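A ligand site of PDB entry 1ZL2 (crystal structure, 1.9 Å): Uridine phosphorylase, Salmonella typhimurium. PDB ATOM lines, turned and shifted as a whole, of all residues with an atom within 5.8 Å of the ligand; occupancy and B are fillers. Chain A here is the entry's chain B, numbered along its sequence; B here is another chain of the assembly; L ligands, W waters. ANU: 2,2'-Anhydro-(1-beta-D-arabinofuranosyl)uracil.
The backbone NH (N) of Met 197 sits close to an oxygen (O2) of the ligand (3.5 Å).
OG1 of Thr 94 is in hydrogen-bond range of O4' of the ligand, at 3.2 Å.
The side-chain carboxylate of Glu 198 lies within hydrogen-bond range of an oxygen (O3') of the ligand (2.6 Å).
NH2 of Arg 168 sits at hydrogen-bond distance from O4 of the ligand (2.9 Å).
OE1 of Gln 166 lies close to O4 of the ligand (3.1 Å).
The guanidinium group (NH2) of Arg 48 of chain B is in hydrogen-bond range of an oxygen (O4') of the ligand, 3.5 Å away.
An oxygen (O5') of the ligand sits at hydrogen-bond distance from a ring nitrogen (NE2) of His 8 of chain B, at 2.6 Å.
The guanidinium group (NE) of Arg 168 sits at hydrogen-bond distance from the backbone carbonyl oxygen (O) of Glu 227, 2.6 Å away.
OE2 of Glu 198 sits at hydrogen-bond distance from N of Gly 70, at 2.7 Å.
NH2 of Arg 91 lies within salt-bridge range of OE1 of Glu 196 (3.1 Å).
OE1 of Glu 196 is in hydrogen-bond range of N of Glu 198 (3.0 Å).
O of Gly 96 sits at hydrogen-bond distance from N of Tyr 195 (2.9 Å).
The backbone carbonyl oxygen (O) of Thr 95 is in hydrogen-bond range of the backbone NH (N) of Ile 220.
O of Gln 166 is in hydrogen-bond range of NH1 of Arg 223, at 2.8 Å.
The side-chain hydroxyl (OG1) of Thr 95 sits at hydrogen-bond distance from the backbone carbonyl oxygen (O) of Tyr 195, 2.5 Å away.
Merely in contact with the ligand: Phe 162 (3.4 Å), Glu 196 (3.6 Å), Gly 96 (3.7 Å), Ile 69 (3.7 Å), Thr 95 (3.8 Å) and Ile 220 (3.8 Å).
Hydrophobic or aromatic side chains within 4 Å of the ligand: Ile 69, Phe 162, Met 197, Ile 220 and His 8 of chain B.
Of the 24 residues printed, 13 come within 4 Å of the ligand.
Along chain A the residues within 4 Å of the ligand span positions 69 to 220.
Water W2 lies within hydrogen-bond range of OE1 of Gln 166 (2.6 Å), O4 of the ligand (2.8 Å), NH1 of Arg 223 (3.0 Å) and NH2 of Arg 168 (3.1 Å).
Water W1 lies within hydrogen-bond range of an oxygen (O5') of the ligand (2.9 Å) and the guanidinium group (NH2) of Arg 48 of chain B (3.1 Å).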
ATOM      1  N   GLY A  26      28.324  13.775  -0.411  1.00  0.00           N
ATOM      2  CA  GLY A  26      29.200  14.924  -0.337  1.00  0.00           C
ATOM      3  C   GLY A  26      28.914  15.773   0.889  1.00  0.00           C
ATOM      4  O   GLY A  26      29.826  16.286   1.525  1.00  0.00           O
ATOM      5  N   GLY A  68      32.781  15.839   1.531  1.00  0.00           N
ATOM      6  CA  GLY A  68      32.952  17.275   1.426  1.00  0.00           C
ATOM      7  C   GLY A  68      32.807  17.545  -0.061  1.00  0.00           C
ATOM      8  O   GLY A  68      32.666  16.606  -0.846  1.00  0.00           O
ATOM      9  N   ILE A  69      32.848  18.804  -0.478  1.00  0.00           N
ATOM     10  CA  ILE A  69      32.728  19.119  -1.900  1.00  0.00           C
ATOM     11  C   ILE A  69      34.082  19.051  -2.592  1.00  0.00           C
ATOM     12  O   ILE A  69      35.080  19.527  -2.065  1.00  0.00           O
ATOM     13  CB  ILE A  69      32.158  20.539  -2.135  1.00  0.00           C
ATOM     14  CG1 ILE A  69      30.687  20.589  -1.720  1.00  0.00           C
ATOM     15  CG2 ILE A  69      32.297  20.916  -3.606  1.00  0.00           C
ATOM     16  CD1 ILE A  69      30.095  21.985  -1.793  1.00  0.00           C
ATOM     17  N   GLY A  70      34.112  18.431  -3.768  1.00  0.00           N
ATOM     18  CA  GLY A  70      35.341  18.371  -4.544  1.00  0.00           C
ATOM     19  C   GLY A  70      36.242  17.167  -4.439  1.00  0.00           C
ATOM     20  O   GLY A  70      36.228  16.416  -3.453  1.00  0.00           O
ATOM     21  N   ARG A  91      29.169   6.542  -4.354  1.00  0.00           N
ATOM     22  CA  ARG A  91      28.896   7.953  -4.138  1.00  0.00           C
ATOM     23  C   ARG A  91      27.444   8.258  -4.465  1.00  0.00           C
ATOM     24  O   ARG A  91      26.916   7.787  -5.475  1.00  0.00           O
ATOM     25  CB  ARG A  91      29.805   8.848  -4.992  1.00  0.00           C
ATOM     26  CG  ARG A  91      29.377  10.319  -4.970  1.00  0.00           C
ATOM     27  CD  ARG A  91      30.418  11.248  -5.610  1.00  0.00           C
ATOM     28  NE  ARG A  91      29.767  12.379  -6.272  1.00  0.00           N
ATOM     29  CZ  ARG A  91      29.084  13.339  -5.642  1.00  0.00           C
ATOM     30  NH1 ARG A  91      28.953  13.323  -4.325  1.00  0.00           N
ATOM     31  NH2 ARG A  91      28.508  14.305  -6.353  1.00  0.00           N
ATOM     32  N   GLY A  93      25.157  11.665  -4.705  1.00  0.00           N
ATOM     33  CA  GLY A  93      25.197  13.116  -4.612  1.00  0.00           C
ATOM     34  C   GLY A  93      24.035  13.819  -5.282  1.00  0.00           C
ATOM     35  O   GLY A  93      22.994  13.218  -5.546  1.00  0.00           O
ATOM     36  N   THR A  94      24.224  15.109  -5.527  1.00  0.00           N
ATOM     37  CA  THR A  94      23.225  15.925  -6.181  1.00  0.00           C
ATOM     38  C   THR A  94      23.883  16.397  -7.466  1.00  0.00           C
ATOM     39  O   THR A  94      25.114  16.474  -7.563  1.00  0.00           O
ATOM     40  CB  THR A  94      22.795  17.123  -5.304  1.00  0.00           C
ATOM     41  OG1 THR A  94      23.942  17.879  -4.905  1.00  0.00           O
ATOM     42  CG2 THR A  94      22.060  16.619  -4.068  1.00  0.00           C
ATOM     43  N   THR A  95      23.080  16.754  -8.463  1.00  0.00           N
ATOM     44  CA  THR A  95      23.651  17.134  -9.733  1.00  0.00           C
ATOM     45  C   THR A  95      22.804  18.084 -10.561  1.00  0.00           C
ATOM     46  O   THR A  95      21.592  18.188 -10.373  1.00  0.00           O
ATOM     47  CB  THR A  95      23.927  15.864 -10.563  1.00  0.00           C
ATOM     48  OG1 THR A  95      24.569  16.202 -11.793  1.00  0.00           O
ATOM     49  CG2 THR A  95      22.612  15.151 -10.876  1.00  0.00           C
ATOM     50  N   GLY A  96      23.461  18.786 -11.481  1.00  0.00           N
ATOM     51  CA  GLY A  96      22.769  19.687 -12.379  1.00  0.00           C
ATOM     52  C   GLY A  96      22.704  19.022 -13.745  1.00  0.00           C
ATOM     53  O   GLY A  96      23.737  18.677 -14.324  1.00  0.00           O
ATOM     54  N   PHE A 162      32.262  24.937  -9.129  1.00  0.00           N
ATOM     55  CA  PHE A 162      30.803  24.927  -9.241  1.00  0.00           C
ATOM     56  C   PHE A 162      30.413  25.973 -10.282  1.00  0.00           C
ATOM     57  O   PHE A 162      29.436  25.819 -11.009  1.00  0.00           O
ATOM     58  CB  PHE A 162      30.183  25.270  -7.886  1.00  0.00           C
ATOM     59  CG  PHE A 162      28.674  25.310  -7.910  1.00  0.00           C
ATOM     60  CD1 PHE A 162      28.003  26.482  -8.220  1.00  0.00           C
ATOM     61  CD2 PHE A 162      27.938  24.184  -7.592  1.00  0.00           C
ATOM     62  CE1 PHE A 162      26.606  26.539  -8.214  1.00  0.00           C
ATOM     63  CE2 PHE A 162      26.546  24.217  -7.578  1.00  0.00           C
ATOM     64  CZ  PHE A 162      25.879  25.397  -7.883  1.00  0.00           C
ATOM     65  N   GLN A 166      31.547  24.842 -14.785  1.00  0.00           N
ATOM     66  CA  GLN A 166      30.246  24.317 -15.198  1.00  0.00           C
ATOM     67  C   GLN A 166      29.575  25.403 -16.030  1.00  0.00           C
ATOM     68  O   GLN A 166      28.353  25.412 -16.227  1.00  0.00           O
ATOM     69  CB  GLN A 166      29.406  23.959 -13.973  1.00  0.00           C
ATOM     70  CG  GLN A 166      30.020  22.837 -13.148  1.00  0.00           C
ATOM     71  CD  GLN A 166      29.116  22.346 -12.042  1.00  0.00           C
ATOM     72  OE1 GLN A 166      27.891  22.324 -12.200  1.00  0.00           O
ATOM     73  NE2 GLN A 166      29.700  21.930 -10.922  1.00  0.00           N
ATOM     74  N   ARG A 168      28.913  28.612 -15.518  1.00  0.00           N
ATOM     75  CA  ARG A 168      27.881  29.439 -14.900  1.00  0.00           C
ATOM     76  C   ARG A 168      28.388  30.877 -15.031  1.00  0.00           C
ATOM     77  O   ARG A 168      29.546  31.162 -14.710  1.00  0.00           O
ATOM     78  CB  ARG A 168      27.692  29.071 -13.425  1.00  0.00           C
ATOM     79  CG  ARG A 168      26.862  27.806 -13.200  1.00  0.00           C
ATOM     80  CD  ARG A 168      26.545  27.597 -11.721  1.00  0.00           C
ATOM     81  NE  ARG A 168      25.464  26.643 -11.516  1.00  0.00           N
ATOM     82  CZ  ARG A 168      25.610  25.356 -11.230  1.00  0.00           C
ATOM     83  NH1 ARG A 168      26.818  24.826 -11.084  1.00  0.00           N
ATOM     84  NH2 ARG A 168      24.531  24.595 -11.090  1.00  0.00           N
ATOM     85  N   TYR A 195      26.379  17.576 -14.530  1.00  0.00           N
ATOM     86  CA  TYR A 195      27.558  18.121 -13.896  1.00  0.00           C
ATOM     87  C   TYR A 195      27.526  17.812 -12.404  1.00  0.00           C
ATOM     88  O   TYR A 195      26.456  17.796 -11.788  1.00  0.00           O
ATOM     89  CB  TYR A 195      27.555  19.667 -13.959  1.00  0.00           C
ATOM     90  CG  TYR A 195      28.061  20.337 -15.203  1.00  0.00           C
ATOM     91  CD1 TYR A 195      29.355  20.105 -15.675  1.00  0.00           C
ATOM     92  CD2 TYR A 195      27.285  21.294 -15.863  1.00  0.00           C
ATOM     93  CE1 TYR A 195      29.859  20.818 -16.767  1.00  0.00           C
ATOM     94  CE2 TYR A 195      27.776  22.010 -16.951  1.00  0.00           C
ATOM     95  CZ  TYR A 195      29.065  21.765 -17.405  1.00  0.00           C
ATOM     96  OH  TYR A 195      29.556  22.476 -18.469  1.00  0.00           O
ATOM     97  N   GLU A 196      28.687  17.533 -11.842  1.00  0.00           N
ATOM     98  CA  GLU A 196      28.841  17.415 -10.393  1.00  0.00           C
ATOM     99  C   GLU A 196      30.324  17.633 -10.176  1.00  0.00           C
ATOM    100  O   GLU A 196      31.031  17.969 -11.140  1.00  0.00           O
ATOM    101  CB  GLU A 196      28.288  16.108  -9.801  1.00  0.00           C
ATOM    102  CG  GLU A 196      28.718  14.853 -10.473  1.00  0.00           C
ATOM    103  CD  GLU A 196      30.095  14.470 -10.037  1.00  0.00           C
ATOM    104  OE1 GLU A 196      30.256  14.101  -8.847  1.00  0.00           O
ATOM    105  OE2 GLU A 196      31.001  14.540 -10.870  1.00  0.00           O
ATOM    106  N   MET A 197      30.837  17.434  -8.970  1.00  0.00           N
ATOM    107  CA  MET A 197      32.236  17.764  -8.719  1.00  0.00           C
ATOM    108  C   MET A 197      33.150  16.734  -8.074  1.00  0.00           C
ATOM    109  O   MET A 197      34.293  17.061  -7.761  1.00  0.00           O
ATOM    110  CB  MET A 197      32.273  19.044  -7.877  1.00  0.00           C
ATOM    111  CG  MET A 197      31.556  20.242  -8.511  1.00  0.00           C
ATOM    112  SD  MET A 197      31.363  21.652  -7.396  1.00  0.00           S
ATOM    113  CE  MET A 197      33.076  22.102  -7.113  1.00  0.00           C
ATOM    114  N   GLU A 198      32.675  15.518  -7.893  1.00  0.00           N
ATOM    115  CA  GLU A 198      33.504  14.513  -7.225  1.00  0.00           C
ATOM    116  C   GLU A 198      33.761  13.205  -7.963  1.00  0.00           C
ATOM    117  O   GLU A 198      34.737  12.507  -7.656  1.00  0.00           O
ATOM    118  CB  GLU A 198      32.900  14.179  -5.854  1.00  0.00           C
ATOM    119  CG  GLU A 198      32.779  15.371  -4.892  1.00  0.00           C
ATOM    120  CD  GLU A 198      31.703  16.375  -5.287  1.00  0.00           C
ATOM    121  OE1 GLU A 198      30.792  16.022  -6.084  1.00  0.00           O
ATOM    122  OE2 GLU A 198      31.759  17.526  -4.807  1.00  0.00           O
ATOM    123  N   ILE A 220      18.993  18.271  -9.112  1.00  0.00           N
ATOM    124  CA  ILE A 220      18.397  19.356  -8.333  1.00  0.00           C
ATOM    125  C   ILE A 220      18.209  20.621  -9.174  1.00  0.00           C
ATOM    126  O   ILE A 220      17.601  21.592  -8.723  1.00  0.00           O
ATOM    127  CB  ILE A 220      19.260  19.702  -7.092  1.00  0.00           C
ATOM    128  CG1 ILE A 220      20.619  20.242  -7.543  1.00  0.00           C
ATOM    129  CG2 ILE A 220      19.419  18.468  -6.221  1.00  0.00           C
ATOM    130  CD1 ILE A 220      21.403  20.888  -6.415  1.00  0.00           C
ATOM    131  N   VAL A 221      18.725  20.611 -10.395  1.00  0.00           N
ATOM    132  CA  VAL A 221      18.583  21.757 -11.289  1.00  0.00           C
ATOM    133  C   VAL A 221      18.853  21.342 -12.726  1.00  0.00           C
ATOM    134  O   VAL A 221      19.683  20.463 -12.989  1.00  0.00           O
ATOM    135  CB  VAL A 221      19.566  22.908 -10.912  1.00  0.00           C
ATOM    136  CG1 VAL A 221      21.015  22.484 -11.163  1.00  0.00           C
ATOM    137  CG2 VAL A 221      19.230  24.154 -11.705  1.00  0.00           C
ATOM    138  N   ARG A 223      20.270  22.788 -16.017  1.00  0.00           N
ATOM    139  CA  ARG A 223      21.053  23.885 -16.565  1.00  0.00           C
ATOM    140  C   ARG A 223      20.608  24.438 -17.921  1.00  0.00           C
ATOM    141  O   ARG A 223      21.054  25.513 -18.318  1.00  0.00           O
ATOM    142  CB  ARG A 223      22.519  23.475 -16.608  1.00  0.00           C
ATOM    143  CG  ARG A 223      23.132  23.236 -15.230  1.00  0.00           C
ATOM    144  CD  ARG A 223      23.197  24.541 -14.436  1.00  0.00           C
ATOM    145  NE  ARG A 223      23.889  25.584 -15.200  1.00  0.00           N
ATOM    146  CZ  ARG A 223      25.190  25.584 -15.449  1.00  0.00           C
ATOM    147  NH1 ARG A 223      25.960  24.605 -14.979  1.00  0.00           N
ATOM    148  NH2 ARG A 223      25.730  26.551 -16.179  1.00  0.00           N
ATOM    149  N   GLU A 227      20.847  28.417 -13.886  1.00  0.00           N
ATOM    150  CA  GLU A 227      22.128  28.050 -13.292  1.00  0.00           C
ATOM    151  C   GLU A 227      22.005  27.483 -11.886  1.00  0.00           C
ATOM    152  O   GLU A 227      22.826  26.663 -11.471  1.00  0.00           O
ATOM    153  CB  GLU A 227      23.068  29.257 -13.277  1.00  0.00           C
ATOM    154  CG  GLU A 227      23.302  29.850 -14.664  1.00  0.00           C
ATOM    155  CD  GLU A 227      24.493  30.774 -14.699  1.00  0.00           C
ATOM    156  OE1 GLU A 227      24.951  31.214 -13.624  1.00  0.00           O
ATOM    157  OE2 GLU A 227      24.972  31.056 -15.828  1.00  0.00           O
ATOM    158  N   PHE B   7      24.066  30.457  -2.987  1.00  0.00           N
ATOM    159  CA  PHE B   7      23.672  29.057  -2.939  1.00  0.00           C
ATOM    160  C   PHE B   7      24.247  28.147  -1.857  1.00  0.00           C
ATOM    161  O   PHE B   7      23.525  27.302  -1.330  1.00  0.00           O
ATOM    162  CB  PHE B   7      23.905  28.415  -4.299  1.00  0.00           C
ATOM    163  CG  PHE B   7      23.246  27.087  -4.461  1.00  0.00           C
ATOM    164  CD1 PHE B   7      21.861  26.959  -4.373  1.00  0.00           C
ATOM    165  CD2 PHE B   7      24.006  25.938  -4.689  1.00  0.00           C
ATOM    166  CE1 PHE B   7      21.239  25.717  -4.510  1.00  0.00           C
ATOM    167  CE2 PHE B   7      23.397  24.693  -4.830  1.00  0.00           C
ATOM    168  CZ  PHE B   7      22.013  24.585  -4.734  1.00  0.00           C
ATOM    169  N   HIS B   8      25.521  28.286  -1.516  1.00  0.00           N
ATOM    170  CA  HIS B   8      26.098  27.401  -0.515  1.00  0.00           C
ATOM    171  C   HIS B   8      26.273  27.969   0.884  1.00  0.00           C
ATOM    172  O   HIS B   8      25.941  27.301   1.865  1.00  0.00           O
ATOM    173  CB  HIS B   8      27.470  26.882  -0.975  1.00  0.00           C
ATOM    174  CG  HIS B   8      27.426  26.092  -2.254  1.00  0.00           C
ATOM    175  ND1 HIS B   8      27.472  26.687  -3.494  1.00  0.00           N
ATOM    176  CD2 HIS B   8      27.314  24.768  -2.473  1.00  0.00           C
ATOM    177  CE1 HIS B   8      27.391  25.758  -4.429  1.00  0.00           C
ATOM    178  NE2 HIS B   8      27.303  24.579  -3.841  1.00  0.00           N
ATOM    179  N   ARG B  48      27.258  22.513   5.055  1.00  0.00           N
ATOM    180  CA  ARG B  48      28.333  21.695   4.516  1.00  0.00           C
ATOM    181  C   ARG B  48      29.620  22.067   5.259  1.00  0.00           C
ATOM    182  O   ARG B  48      29.597  22.210   6.486  1.00  0.00           O
ATOM    183  CB  ARG B  48      28.486  21.927   3.009  1.00  0.00           C
ATOM    184  CG  ARG B  48      27.330  21.340   2.175  1.00  0.00           C
ATOM    185  CD  ARG B  48      27.428  21.786   0.712  1.00  0.00           C
ATOM    186  NE  ARG B  48      26.450  21.152  -0.175  1.00  0.00           N
ATOM    187  CZ  ARG B  48      26.605  19.955  -0.747  1.00  0.00           C
ATOM    188  NH1 ARG B  48      27.703  19.234  -0.540  1.00  0.00           N
ATOM    189  NH2 ARG B  48      25.653  19.473  -1.549  1.00  0.00           N
ATOM    190  N   ILE B  76      34.201  27.928  -4.177  1.00  0.00           N
ATOM    191  CA  ILE B  76      32.804  28.228  -3.909  1.00  0.00           C
ATOM    192  C   ILE B  76      32.698  29.314  -2.844  1.00  0.00           C
ATOM    193  O   ILE B  76      32.029  30.327  -3.030  1.00  0.00           O
ATOM    194  CB  ILE B  76      32.037  26.982  -3.410  1.00  0.00           C
ATOM    195  CG1 ILE B  76      31.914  25.964  -4.550  1.00  0.00           C
ATOM    196  CG2 ILE B  76      30.662  27.379  -2.868  1.00  0.00           C
ATOM    197  CD1 ILE B  76      31.289  24.630  -4.134  1.00  0.00           C
HETATM  198  O3' ANU L   1      29.369  18.276  -4.315  1.00  0.00           O
HETATM  199  C3' ANU L   1      29.039  19.320  -5.240  1.00  0.00           C
HETATM  200  C2' ANU L   1      28.360  18.723  -6.477  1.00  0.00           C
HETATM  201  O2  ANU L   1      28.532  19.633  -7.567  1.00  0.00           O
HETATM  202  C2  ANU L   1      27.316  20.006  -8.040  1.00  0.00           C
HETATM  203  N3  ANU L   1      26.974  20.802  -9.145  1.00  0.00           N
HETATM  204  C4  ANU L   1      25.644  21.158  -9.393  1.00  0.00           C
HETATM  205  O4  ANU L   1      25.383  21.899 -10.348  1.00  0.00           O
HETATM  206  C5  ANU L   1      24.635  20.717  -8.553  1.00  0.00           C
HETATM  207  C6  ANU L   1      24.953  19.924  -7.453  1.00  0.00           C
HETATM  208  N1  ANU L   1      26.288  19.565  -7.189  1.00  0.00           N
HETATM  209  C1' ANU L   1      26.878  18.725  -6.132  1.00  0.00           C
HETATM  210  O4' ANU L   1      26.748  19.339  -4.836  1.00  0.00           O
HETATM  211  C4' ANU L   1      27.916  20.155  -4.625  1.00  0.00           C
HETATM  212  C5' ANU L   1      27.764  21.502  -5.350  1.00  0.00           C
HETATM  213  O5' ANU L   1      26.671  22.225  -4.770  1.00  0.00           O
HETATM  214  O   HOH W   1      24.193  21.378  -3.472  1.00  0.00           O
HETATM  215  O   HOH W   2      25.403  22.320 -13.082  1.00  0.00           O
